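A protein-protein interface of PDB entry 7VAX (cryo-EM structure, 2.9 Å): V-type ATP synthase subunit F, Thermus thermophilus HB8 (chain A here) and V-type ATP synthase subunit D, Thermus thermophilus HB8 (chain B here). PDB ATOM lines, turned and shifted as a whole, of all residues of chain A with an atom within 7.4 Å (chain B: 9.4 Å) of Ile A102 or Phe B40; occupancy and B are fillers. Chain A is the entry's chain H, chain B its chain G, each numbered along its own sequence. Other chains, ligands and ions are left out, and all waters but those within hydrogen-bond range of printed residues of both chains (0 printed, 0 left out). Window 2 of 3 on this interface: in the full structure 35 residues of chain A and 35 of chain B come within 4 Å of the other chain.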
ATOM      1  N   ARG A  91      -5.803 -24.903  33.288  1.00  0.00           N
ATOM      2  CA  ARG A  91      -7.021 -25.703  33.308  1.00  0.00           C
ATOM      3  C   ARG A  91      -8.259 -24.818  33.323  1.00  0.00           C
ATOM      4  O   ARG A  91      -9.239 -25.097  32.623  1.00  0.00           O
ATOM      5  CB  ARG A  91      -7.012 -26.637  34.518  1.00  0.00           C
ATOM      6  CG  ARG A  91      -8.189 -27.592  34.580  1.00  0.00           C
ATOM      7  CD  ARG A  91      -8.044 -28.560  35.741  1.00  0.00           C
ATOM      8  NE  ARG A  91      -9.079 -29.588  35.726  1.00  0.00           N
ATOM      9  CZ  ARG A  91      -8.874 -30.858  36.044  1.00  0.00           C
ATOM     10  NH1 ARG A  91      -7.681 -31.296  36.413  1.00  0.00           N
ATOM     11  NH2 ARG A  91      -9.893 -31.712  35.992  1.00  0.00           N
ATOM     12  N   VAL A  94      -8.687 -23.316  29.828  1.00  0.00           N
ATOM     13  CA  VAL A  94      -9.176 -24.319  28.886  1.00  0.00           C
ATOM     14  C   VAL A  94     -10.653 -24.600  29.125  1.00  0.00           C
ATOM     15  O   VAL A  94     -11.447 -24.676  28.179  1.00  0.00           O
ATOM     16  CB  VAL A  94      -8.328 -25.601  28.987  1.00  0.00           C
ATOM     17  CG1 VAL A  94      -9.030 -26.760  28.300  1.00  0.00           C
ATOM     18  CG2 VAL A  94      -6.952 -25.373  28.381  1.00  0.00           C
ATOM     19  N   ARG A  95     -11.048 -24.753  30.391  1.00  0.00           N
ATOM     20  CA  ARG A  95     -12.447 -25.017  30.705  1.00  0.00           C
ATOM     21  C   ARG A  95     -13.340 -23.844  30.321  1.00  0.00           C
ATOM     22  O   ARG A  95     -14.499 -24.047  29.946  1.00  0.00           O
ATOM     23  CB  ARG A  95     -12.595 -25.340  32.192  1.00  0.00           C
ATOM     24  CG  ARG A  95     -13.805 -26.193  32.530  1.00  0.00           C
ATOM     25  CD  ARG A  95     -14.508 -25.685  33.777  1.00  0.00           C
ATOM     26  NE  ARG A  95     -15.061 -24.350  33.586  1.00  0.00           N
ATOM     27  CZ  ARG A  95     -16.218 -24.097  32.989  1.00  0.00           C
ATOM     28  NH1 ARG A  95     -16.978 -25.070  32.514  1.00  0.00           N
ATOM     29  NH2 ARG A  95     -16.622 -22.837  32.864  1.00  0.00           N
ATOM     30  N   ILE A  98     -13.484 -23.784  26.291  1.00  0.00           N
ATOM     31  CA  ILE A  98     -14.074 -24.968  25.689  1.00  0.00           C
ATOM     32  C   ILE A  98     -15.428 -25.318  26.300  1.00  0.00           C
ATOM     33  O   ILE A  98     -16.292 -25.855  25.595  1.00  0.00           O
ATOM     34  CB  ILE A  98     -13.103 -26.166  25.787  1.00  0.00           C
ATOM     35  CG1 ILE A  98     -11.756 -25.815  25.155  1.00  0.00           C
ATOM     36  CG2 ILE A  98     -13.682 -27.398  25.106  1.00  0.00           C
ATOM     37  CD1 ILE A  98     -11.863 -25.282  23.742  1.00  0.00           C
ATOM     38  N   GLY A  99     -15.653 -25.004  27.573  1.00  0.00           N
ATOM     39  CA  GLY A  99     -16.888 -25.355  28.238  1.00  0.00           C
ATOM     40  C   GLY A  99     -16.907 -26.724  28.879  1.00  0.00           C
ATOM     41  O   GLY A  99     -17.936 -27.105  29.450  1.00  0.00           O
ATOM     42  N   PHE A 100     -15.810 -27.474  28.807  1.00  0.00           N
ATOM     43  CA  PHE A 100     -15.727 -28.799  29.399  1.00  0.00           C
ATOM     44  C   PHE A 100     -14.452 -28.911  30.223  1.00  0.00           C
ATOM     45  O   PHE A 100     -13.426 -28.310  29.894  1.00  0.00           O
ATOM     46  CB  PHE A 100     -15.755 -29.897  28.328  1.00  0.00           C
ATOM     47  CG  PHE A 100     -17.032 -29.942  27.540  1.00  0.00           C
ATOM     48  CD1 PHE A 100     -17.190 -29.164  26.406  1.00  0.00           C
ATOM     49  CD2 PHE A 100     -18.075 -30.764  27.934  1.00  0.00           C
ATOM     50  CE1 PHE A 100     -18.364 -29.203  25.678  1.00  0.00           C
ATOM     51  CE2 PHE A 100     -19.252 -30.807  27.211  1.00  0.00           C
ATOM     52  CZ  PHE A 100     -19.396 -30.025  26.081  1.00  0.00           C
ATOM     53  N   ASP A 101     -14.529 -29.689  31.299  1.00  0.00           N
ATOM     54  CA  ASP A 101     -13.395 -29.902  32.192  1.00  0.00           C
ATOM     55  C   ASP A 101     -12.629 -31.132  31.716  1.00  0.00           C
ATOM     56  O   ASP A 101     -13.143 -32.254  31.775  1.00  0.00           O
ATOM     57  CB  ASP A 101     -13.869 -30.068  33.634  1.00  0.00           C
ATOM     58  CG  ASP A 101     -12.721 -30.137  34.619  1.00  0.00           C
ATOM     59  OD1 ASP A 101     -11.764 -29.349  34.475  1.00  0.00           O
ATOM     60  OD2 ASP A 101     -12.777 -30.979  35.540  1.00  0.00           O
ATOM     61  N   ILE A 102     -11.398 -30.922  31.249  1.00  0.00           N
ATOM     62  CA  ILE A 102     -10.584 -31.982  30.673  1.00  0.00           C
ATOM     63  C   ILE A 102      -9.210 -31.973  31.327  1.00  0.00           C
ATOM     64  O   ILE A 102      -8.787 -30.986  31.931  1.00  0.00           O
ATOM     65  CB  ILE A 102     -10.449 -31.842  29.141  1.00  0.00           C
ATOM     66  CG1 ILE A 102      -9.722 -30.543  28.791  1.00  0.00           C
ATOM     67  CG2 ILE A 102     -11.815 -31.892  28.474  1.00  0.00           C
ATOM     68  CD1 ILE A 102      -9.600 -30.297  27.307  1.00  0.00           C
ATOM     69  N   LYS A 103      -8.514 -33.099  31.194  1.00  0.00           N
ATOM     70  CA  LYS A 103      -7.176 -33.242  31.751  1.00  0.00           C
ATOM     71  C   LYS A 103      -6.144 -32.646  30.803  1.00  0.00           C
ATOM     72  O   LYS A 103      -6.184 -32.890  29.593  1.00  0.00           O
ATOM     73  CB  LYS A 103      -6.863 -34.715  32.012  1.00  0.00           C
ATOM     74  CG  LYS A 103      -5.429 -34.991  32.424  1.00  0.00           C
ATOM     75  CD  LYS A 103      -5.200 -36.477  32.643  1.00  0.00           C
ATOM     76  CE  LYS A 103      -5.616 -37.282  31.421  1.00  0.00           C
ATOM     77  NZ  LYS A 103      -4.717 -37.040  30.259  1.00  0.00           N
ATOM     78  N   LEU A 104      -5.220 -31.866  31.354  1.00  0.00           N
ATOM     79  CA  LEU A 104      -4.152 -31.269  30.562  1.00  0.00           C
ATOM     80  C   LEU A 104      -2.845 -32.032  30.749  1.00  0.00           C
ATOM     81  O   LEU A 104      -2.642 -32.695  31.766  1.00  0.00           O
ATOM     82  CB  LEU A 104      -3.962 -29.799  30.938  1.00  0.00           C
ATOM     83  CG  LEU A 104      -5.138 -28.870  30.633  1.00  0.00           C
ATOM     84  CD1 LEU A 104      -4.776 -27.430  30.950  1.00  0.00           C
ATOM     85  CD2 LEU A 104      -5.571 -29.013  29.183  1.00  0.00           C
ATOM     86  N   ARG B  32     -13.056 -29.421  13.095  1.00  0.00           N
ATOM     87  CA  ARG B  32     -13.021 -29.209  14.537  1.00  0.00           C
ATOM     88  C   ARG B  32     -12.002 -30.120  15.204  1.00  0.00           C
ATOM     89  O   ARG B  32     -11.330 -29.715  16.156  1.00  0.00           O
ATOM     90  CB  ARG B  32     -14.408 -29.433  15.132  1.00  0.00           C
ATOM     91  CG  ARG B  32     -14.523 -29.065  16.598  1.00  0.00           C
ATOM     92  CD  ARG B  32     -15.943 -29.260  17.089  1.00  0.00           C
ATOM     93  NE  ARG B  32     -16.331 -30.665  17.071  1.00  0.00           N
ATOM     94  CZ  ARG B  32     -17.546 -31.109  17.355  1.00  0.00           C
ATOM     95  NH1 ARG B  32     -18.525 -30.282  17.682  1.00  0.00           N
ATOM     96  NH2 ARG B  32     -17.785 -32.417  17.312  1.00  0.00           N
ATOM     97  N   ASP B  33     -11.885 -31.363  14.732  1.00  0.00           N
ATOM     98  CA  ASP B  33     -10.875 -32.263  15.286  1.00  0.00           C
ATOM     99  C   ASP B  33      -9.468 -31.728  15.043  1.00  0.00           C
ATOM    100  O   ASP B  33      -8.619 -31.745  15.947  1.00  0.00           O
ATOM    101  CB  ASP B  33     -11.030 -33.660  14.685  1.00  0.00           C
ATOM    102  CG  ASP B  33     -12.291 -34.358  15.152  1.00  0.00           C
ATOM    103  OD1 ASP B  33     -12.935 -33.854  16.097  1.00  0.00           O
ATOM    104  OD2 ASP B  33     -12.638 -35.411  14.579  1.00  0.00           O
ATOM    105  N   ALA B  34      -9.204 -31.242  13.827  1.00  0.00           N
ATOM    106  CA  ALA B  34      -7.895 -30.653  13.548  1.00  0.00           C
ATOM    107  C   ALA B  34      -7.645 -29.427  14.422  1.00  0.00           C
ATOM    108  O   ALA B  34      -6.541 -29.240  14.959  1.00  0.00           O
ATOM    109  CB  ALA B  34      -7.783 -30.294  12.068  1.00  0.00           C
ATOM    110  N   LEU B  35      -8.668 -28.584  14.582  1.00  0.00           N
ATOM    111  CA  LEU B  35      -8.541 -27.403  15.429  1.00  0.00           C
ATOM    112  C   LEU B  35      -8.273 -27.789  16.878  1.00  0.00           C
ATOM    113  O   LEU B  35      -7.513 -27.110  17.573  1.00  0.00           O
ATOM    114  CB  LEU B  35      -9.803 -26.550  15.326  1.00  0.00           C
ATOM    115  CG  LEU B  35      -9.804 -25.463  14.252  1.00  0.00           C
ATOM    116  CD1 LEU B  35     -11.145 -24.754  14.213  1.00  0.00           C
ATOM    117  CD2 LEU B  35      -8.683 -24.473  14.505  1.00  0.00           C
ATOM    118  N   VAL B  36      -8.888 -28.874  17.350  1.00  0.00           N
ATOM    119  CA  VAL B  36      -8.679 -29.317  18.725  1.00  0.00           C
ATOM    120  C   VAL B  36      -7.257 -29.832  18.914  1.00  0.00           C
ATOM    121  O   VAL B  36      -6.627 -29.589  19.951  1.00  0.00           O
ATOM    122  CB  VAL B  36      -9.730 -30.377  19.102  1.00  0.00           C
ATOM    123  CG1 VAL B  36      -9.290 -31.165  20.322  1.00  0.00           C
ATOM    124  CG2 VAL B  36     -11.074 -29.716  19.359  1.00  0.00           C
ATOM    125  N   ALA B  37      -6.728 -30.554  17.923  1.00  0.00           N
ATOM    126  CA  ALA B  37      -5.336 -30.992  18.004  1.00  0.00           C
ATOM    127  C   ALA B  37      -4.392 -29.795  18.081  1.00  0.00           C
ATOM    128  O   ALA B  37      -3.477 -29.751  18.921  1.00  0.00           O
ATOM    129  CB  ALA B  37      -4.994 -31.876  16.805  1.00  0.00           C
ATOM    130  N   GLU B  38      -4.616 -28.800  17.217  1.00  0.00           N
ATOM    131  CA  GLU B  38      -3.811 -27.583  17.273  1.00  0.00           C
ATOM    132  C   GLU B  38      -3.959 -26.889  18.622  1.00  0.00           C
ATOM    133  O   GLU B  38      -2.980 -26.379  19.183  1.00  0.00           O
ATOM    134  CB  GLU B  38      -4.205 -26.641  16.136  1.00  0.00           C
ATOM    135  CG  GLU B  38      -3.352 -25.388  16.039  1.00  0.00           C
ATOM    136  CD  GLU B  38      -2.081 -25.609  15.242  1.00  0.00           C
ATOM    137  OE1 GLU B  38      -2.052 -26.545  14.416  1.00  0.00           O
ATOM    138  OE2 GLU B  38      -1.112 -24.847  15.442  1.00  0.00           O
ATOM    139  N   PHE B  39      -5.179 -26.862  19.158  1.00  0.00           N
ATOM    140  CA  PHE B  39      -5.429 -26.226  20.445  1.00  0.00           C
ATOM    141  C   PHE B  39      -4.642 -26.904  21.555  1.00  0.00           C
ATOM    142  O   PHE B  39      -4.070 -26.231  22.414  1.00  0.00           O
ATOM    143  CB  PHE B  39      -6.926 -26.251  20.749  1.00  0.00           C
ATOM    144  CG  PHE B  39      -7.286 -25.697  22.097  1.00  0.00           C
ATOM    145  CD1 PHE B  39      -7.475 -24.336  22.271  1.00  0.00           C
ATOM    146  CD2 PHE B  39      -7.462 -26.536  23.184  1.00  0.00           C
ATOM    147  CE1 PHE B  39      -7.814 -23.824  23.508  1.00  0.00           C
ATOM    148  CE2 PHE B  39      -7.801 -26.030  24.421  1.00  0.00           C
ATOM    149  CZ  PHE B  39      -7.977 -24.672  24.583  1.00  0.00           C
ATOM    150  N   PHE B  40      -4.606 -28.236  21.558  1.00  0.00           N
ATOM    151  CA  PHE B  40      -3.848 -28.942  22.588  1.00  0.00           C
ATOM    152  C   PHE B  40      -2.352 -28.676  22.457  1.00  0.00           C
ATOM    153  O   PHE B  40      -1.652 -28.507  23.467  1.00  0.00           O
ATOM    154  CB  PHE B  40      -4.142 -30.438  22.530  1.00  0.00           C
ATOM    155  CG  PHE B  40      -5.470 -30.811  23.115  1.00  0.00           C
ATOM    156  CD1 PHE B  40      -5.977 -30.114  24.199  1.00  0.00           C
ATOM    157  CD2 PHE B  40      -6.210 -31.853  22.590  1.00  0.00           C
ATOM    158  CE1 PHE B  40      -7.198 -30.447  24.744  1.00  0.00           C
ATOM    159  CE2 PHE B  40      -7.433 -32.194  23.134  1.00  0.00           C
ATOM    160  CZ  PHE B  40      -7.927 -31.488  24.213  1.00  0.00           C
ATOM    161  N   GLY B  41      -1.843 -28.633  21.223  1.00  0.00           N
ATOM    162  CA  GLY B  41      -0.443 -28.270  21.039  1.00  0.00           C
ATOM    163  C   GLY B  41      -0.129 -26.892  21.598  1.00  0.00           C
ATOM    164  O   GLY B  41       0.860 -26.702  22.322  1.00  0.00           O
ATOM    165  N   LEU B  42      -0.981 -25.913  21.285  1.00  0.00           N
ATOM    166  CA  LEU B  42      -0.789 -24.570  21.819  1.00  0.00           C
ATOM    167  C   LEU B  42      -0.950 -24.525  23.333  1.00  0.00           C
ATOM    168  O   LEU B  42      -0.295 -23.715  23.991  1.00  0.00           O
ATOM    169  CB  LEU B  42      -1.745 -23.580  21.152  1.00  0.00           C
ATOM    170  CG  LEU B  42      -1.307 -22.926  19.838  1.00  0.00           C
ATOM    171  CD1 LEU B  42      -1.272 -23.894  18.673  1.00  0.00           C
ATOM    172  CD2 LEU B  42      -2.233 -21.763  19.530  1.00  0.00           C
ATOM    173  N   VAL B  43      -1.809 -25.369  23.906  1.00  0.00           N
ATOM    174  CA  VAL B  43      -1.939 -25.409  25.363  1.00  0.00           C
ATOM    175  C   VAL B  43      -0.649 -25.902  26.003  1.00  0.00           C
ATOM    176  O   VAL B  43      -0.198 -25.361  27.020  1.00  0.00           O
ATOM    177  CB  VAL B  43      -3.146 -26.271  25.782  1.00  0.00           C
ATOM    178  CG1 VAL B  43      -3.150 -26.469  27.285  1.00  0.00           C
ATOM    179  CG2 VAL B  43      -4.435 -25.597  25.373  1.00  0.00           C
ATOM    180  N   ARG B  44      -0.039 -26.940  25.429  1.00  0.00           N
ATOM    181  CA  ARG B  44       1.236 -27.417  25.963  1.00  0.00           C
ATOM    182  C   ARG B  44       2.310 -26.337  25.862  1.00  0.00           C
ATOM    183  O   ARG B  44       3.064 -26.090  26.820  1.00  0.00           O
ATOM    184  CB  ARG B  44       1.674 -28.686  25.232  1.00  0.00           C
ATOM    185  CG  ARG B  44       0.904 -29.931  25.638  1.00  0.00           C
ATOM    186  CD  ARG B  44       1.414 -31.159  24.903  1.00  0.00           C
ATOM    187  NE  ARG B  44       0.727 -32.374  25.325  1.00  0.00           N
ATOM    188  CZ  ARG B  44      -0.482 -32.734  24.915  1.00  0.00           C
ATOM    189  NH1 ARG B  44      -1.172 -31.993  24.062  1.00  0.00           N
ATOM    190  NH2 ARG B  44      -1.012 -33.864  25.373  1.00  0.00           N
ATOM    191  N   GLU B  45       2.388 -25.670  24.707  1.00  0.00           N
ATOM    192  CA  GLU B  45       3.383 -24.613  24.552  1.00  0.00           C
ATOM    193  C   GLU B  45       3.110 -23.456  25.508  1.00  0.00           C
ATOM    194  O   GLU B  45       4.045 -22.847  26.042  1.00  0.00           O
ATOM    195  CB  GLU B  45       3.418 -24.128  23.103  1.00  0.00           C
ATOM    196  CG  GLU B  45       4.713 -23.426  22.717  1.00  0.00           C
ATOM    197  CD  GLU B  45       4.671 -21.932  22.957  1.00  0.00           C
ATOM    198  OE1 GLU B  45       3.571 -21.350  22.883  1.00  0.00           O
ATOM    199  OE2 GLU B  45       5.739 -21.339  23.218  1.00  0.00           O
ATOM    200  N   ALA B  46       1.832 -23.149  25.745  1.00  0.00           N
ATOM    201  CA  ALA B  46       1.467 -22.099  26.688  1.00  0.00           C
ATOM    202  C   ALA B  46       1.867 -22.465  28.107  1.00  0.00           C
ATOM    203  O   ALA B  46       2.308 -21.606  28.873  1.00  0.00           O
ATOM    204  CB  ALA B  46      -0.035 -21.826  26.615  1.00  0.00           C
ATOM    205  N   MET B  47       1.693 -23.732  28.488  1.00  0.00           N
ATOM    206  CA  MET B  47       2.130 -24.167  29.810  1.00  0.00           C
ATOM    207  C   MET B  47       3.636 -23.997  29.969  1.00  0.00           C
ATOM    208  O   MET B  47       4.111 -23.498  31.001  1.00  0.00           O
ATOM    209  CB  MET B  47       1.728 -25.621  30.047  1.00  0.00           C
ATOM    210  CG  MET B  47       0.412 -25.793  30.780  1.00  0.00           C
ATOM    211  SD  MET B  47       0.047 -27.521  31.140  1.00  0.00           S
ATOM    212  CE  MET B  47      -1.274 -27.347  32.336  1.00  0.00           C
ATOM    213  N   GLU B  48       4.402 -24.398  28.950  1.00  0.00           N
ATOM    214  CA  GLU B  48       5.851 -24.217  29.018  1.00  0.00           C
ATOM    215  C   GLU B  48       6.218 -22.739  29.132  1.00  0.00           C
ATOM    216  O   GLU B  48       7.071 -22.360  29.951  1.00  0.00           O
ATOM    217  CB  GLU B  48       6.518 -24.843  27.794  1.00  0.00           C
ATOM    218  CG  GLU B  48       7.992 -25.155  27.989  1.00  0.00           C
ATOM    219  CD  GLU B  48       8.591 -25.912  26.820  1.00  0.00           C
ATOM    220  OE1 GLU B  48       8.104 -27.023  26.516  1.00  0.00           O
ATOM    221  OE2 GLU B  48       9.549 -25.400  26.205  1.00  0.00           O
ATOM    222  N   THR B 143       1.633 -16.235  22.761  1.00  0.00           N
ATOM    223  CA  THR B 143       1.030 -17.565  22.775  1.00  0.00           C
ATOM    224  C   THR B 143      -0.448 -17.505  23.150  1.00  0.00           C
ATOM    225  O   THR B 143      -1.284 -18.169  22.523  1.00  0.00           O
ATOM    226  CB  THR B 143       1.788 -18.473  23.740  1.00  0.00           C
ATOM    227  OG1 THR B 143       3.099 -18.735  23.221  1.00  0.00           O
ATOM    228  CG2 THR B 143       1.049 -19.784  23.910  1.00  0.00           C
ATOM    229  N   LEU B 147      -3.897 -18.816  21.310  1.00  0.00           N
ATOM    230  CA  LEU B 147      -4.726 -19.811  21.984  1.00  0.00           C
ATOM    231  C   LEU B 147      -6.178 -19.353  22.074  1.00  0.00           C
ATOM    232  O   LEU B 147      -7.103 -20.137  21.828  1.00  0.00           O
ATOM    233  CB  LEU B 147      -4.168 -20.098  23.377  1.00  0.00           C
ATOM    234  CG  LEU B 147      -4.709 -21.337  24.089  1.00  0.00           C
ATOM    235  CD1 LEU B 147      -4.484 -22.575  23.244  1.00  0.00           C
ATOM    236  CD2 LEU B 147      -4.052 -21.495  25.449  1.00  0.00           C
ATOM    237  N   ILE B 150      -7.790 -19.591  18.644  1.00  0.00           N
ATOM    238  CA  ILE B 150      -8.087 -20.980  18.308  1.00  0.00           C
ATOM    239  C   ILE B 150      -9.320 -21.455  19.066  1.00  0.00           C
ATOM    240  O   ILE B 150     -10.174 -22.161  18.514  1.00  0.00           O
ATOM    241  CB  ILE B 150      -6.864 -21.872  18.590  1.00  0.00           C
ATOM    242  CG1 ILE B 150      -5.786 -21.645  17.528  1.00  0.00           C
ATOM    243  CG2 ILE B 150      -7.264 -23.336  18.634  1.00  0.00           C
ATOM    244  CD1 ILE B 150      -6.078 -22.318  16.207  1.00  0.00           C
ATOM    245  N   GLY B 151      -9.432 -21.076  20.340  1.00  0.00           N
ATOM    246  CA  GLY B 151     -10.633 -21.403  21.092  1.00  0.00           C
ATOM    247  C   GLY B 151     -11.881 -20.779  20.497  1.00  0.00           C
ATOM    248  O   GLY B 151     -12.941 -21.408  20.451  1.00  0.00           O
ATOM    249  N   ILE B 154     -12.802 -22.808  17.470  1.00  0.00           N
ATOM    250  CA  ILE B 154     -13.405 -24.074  17.876  1.00  0.00           C
ATOM    251  C   ILE B 154     -14.846 -23.858  18.315  1.00  0.00           C
ATOM    252  O   ILE B 154     -15.741 -24.640  17.972  1.00  0.00           O
ATOM    253  CB  ILE B 154     -12.566 -24.740  18.982  1.00  0.00           C
ATOM    254  CG1 ILE B 154     -11.307 -25.367  18.386  1.00  0.00           C
ATOM    255  CG2 ILE B 154     -13.380 -25.791  19.719  1.00  0.00           C
ATOM    256  CD1 ILE B 154     -10.296 -25.796  19.418  1.00  0.00           C
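Among the printed residues, merely in contact across the chains: Ile A102 with Phe B40, Leu A104 with Met B47, Val A94 with Val B43, Ile A98 with Phe B39, Leu A104 with Val B43 and Val A94 with Phe B39.
Of the printed residues of chain B, Ile A102 touches Phe B40 (3.5 Å).
Phe B40 touches just one residue of chain A: Ile A102 (3.5 Å).
No residue of chain A comes within 4 Å of Gly B41.
Of the printed residues of chain A, Met B47 touches Leu A104 (3.8 Å).
Of the printed residues of chain A, Val B43 touches Val A94 and Leu A104.
Of the printed residues of chain A, Phe B39 touches Val A94 (3.996 Å) and Ile A98 (3.99 Å).
Printed residues of chain B within 4 Å of Leu A104: Val B43 and Met B47.
The nearest residue of chain B that does not touch Ile A102 is Phe B39 (5.5 Å).
The nearest residue of chain A that does not touch Phe B40 is Leu A104 (4.9 Å).
Hydrophobic or aromatic side chains of chain B within 4 Å of the printed part of chain A: Phe B39, Phe B40, Val B43 and Met B47.
Among the printed residues, no Asp or Glu carboxylate lies within 4 Å of a Lys or Arg side-chain nitrogen of the other chain.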
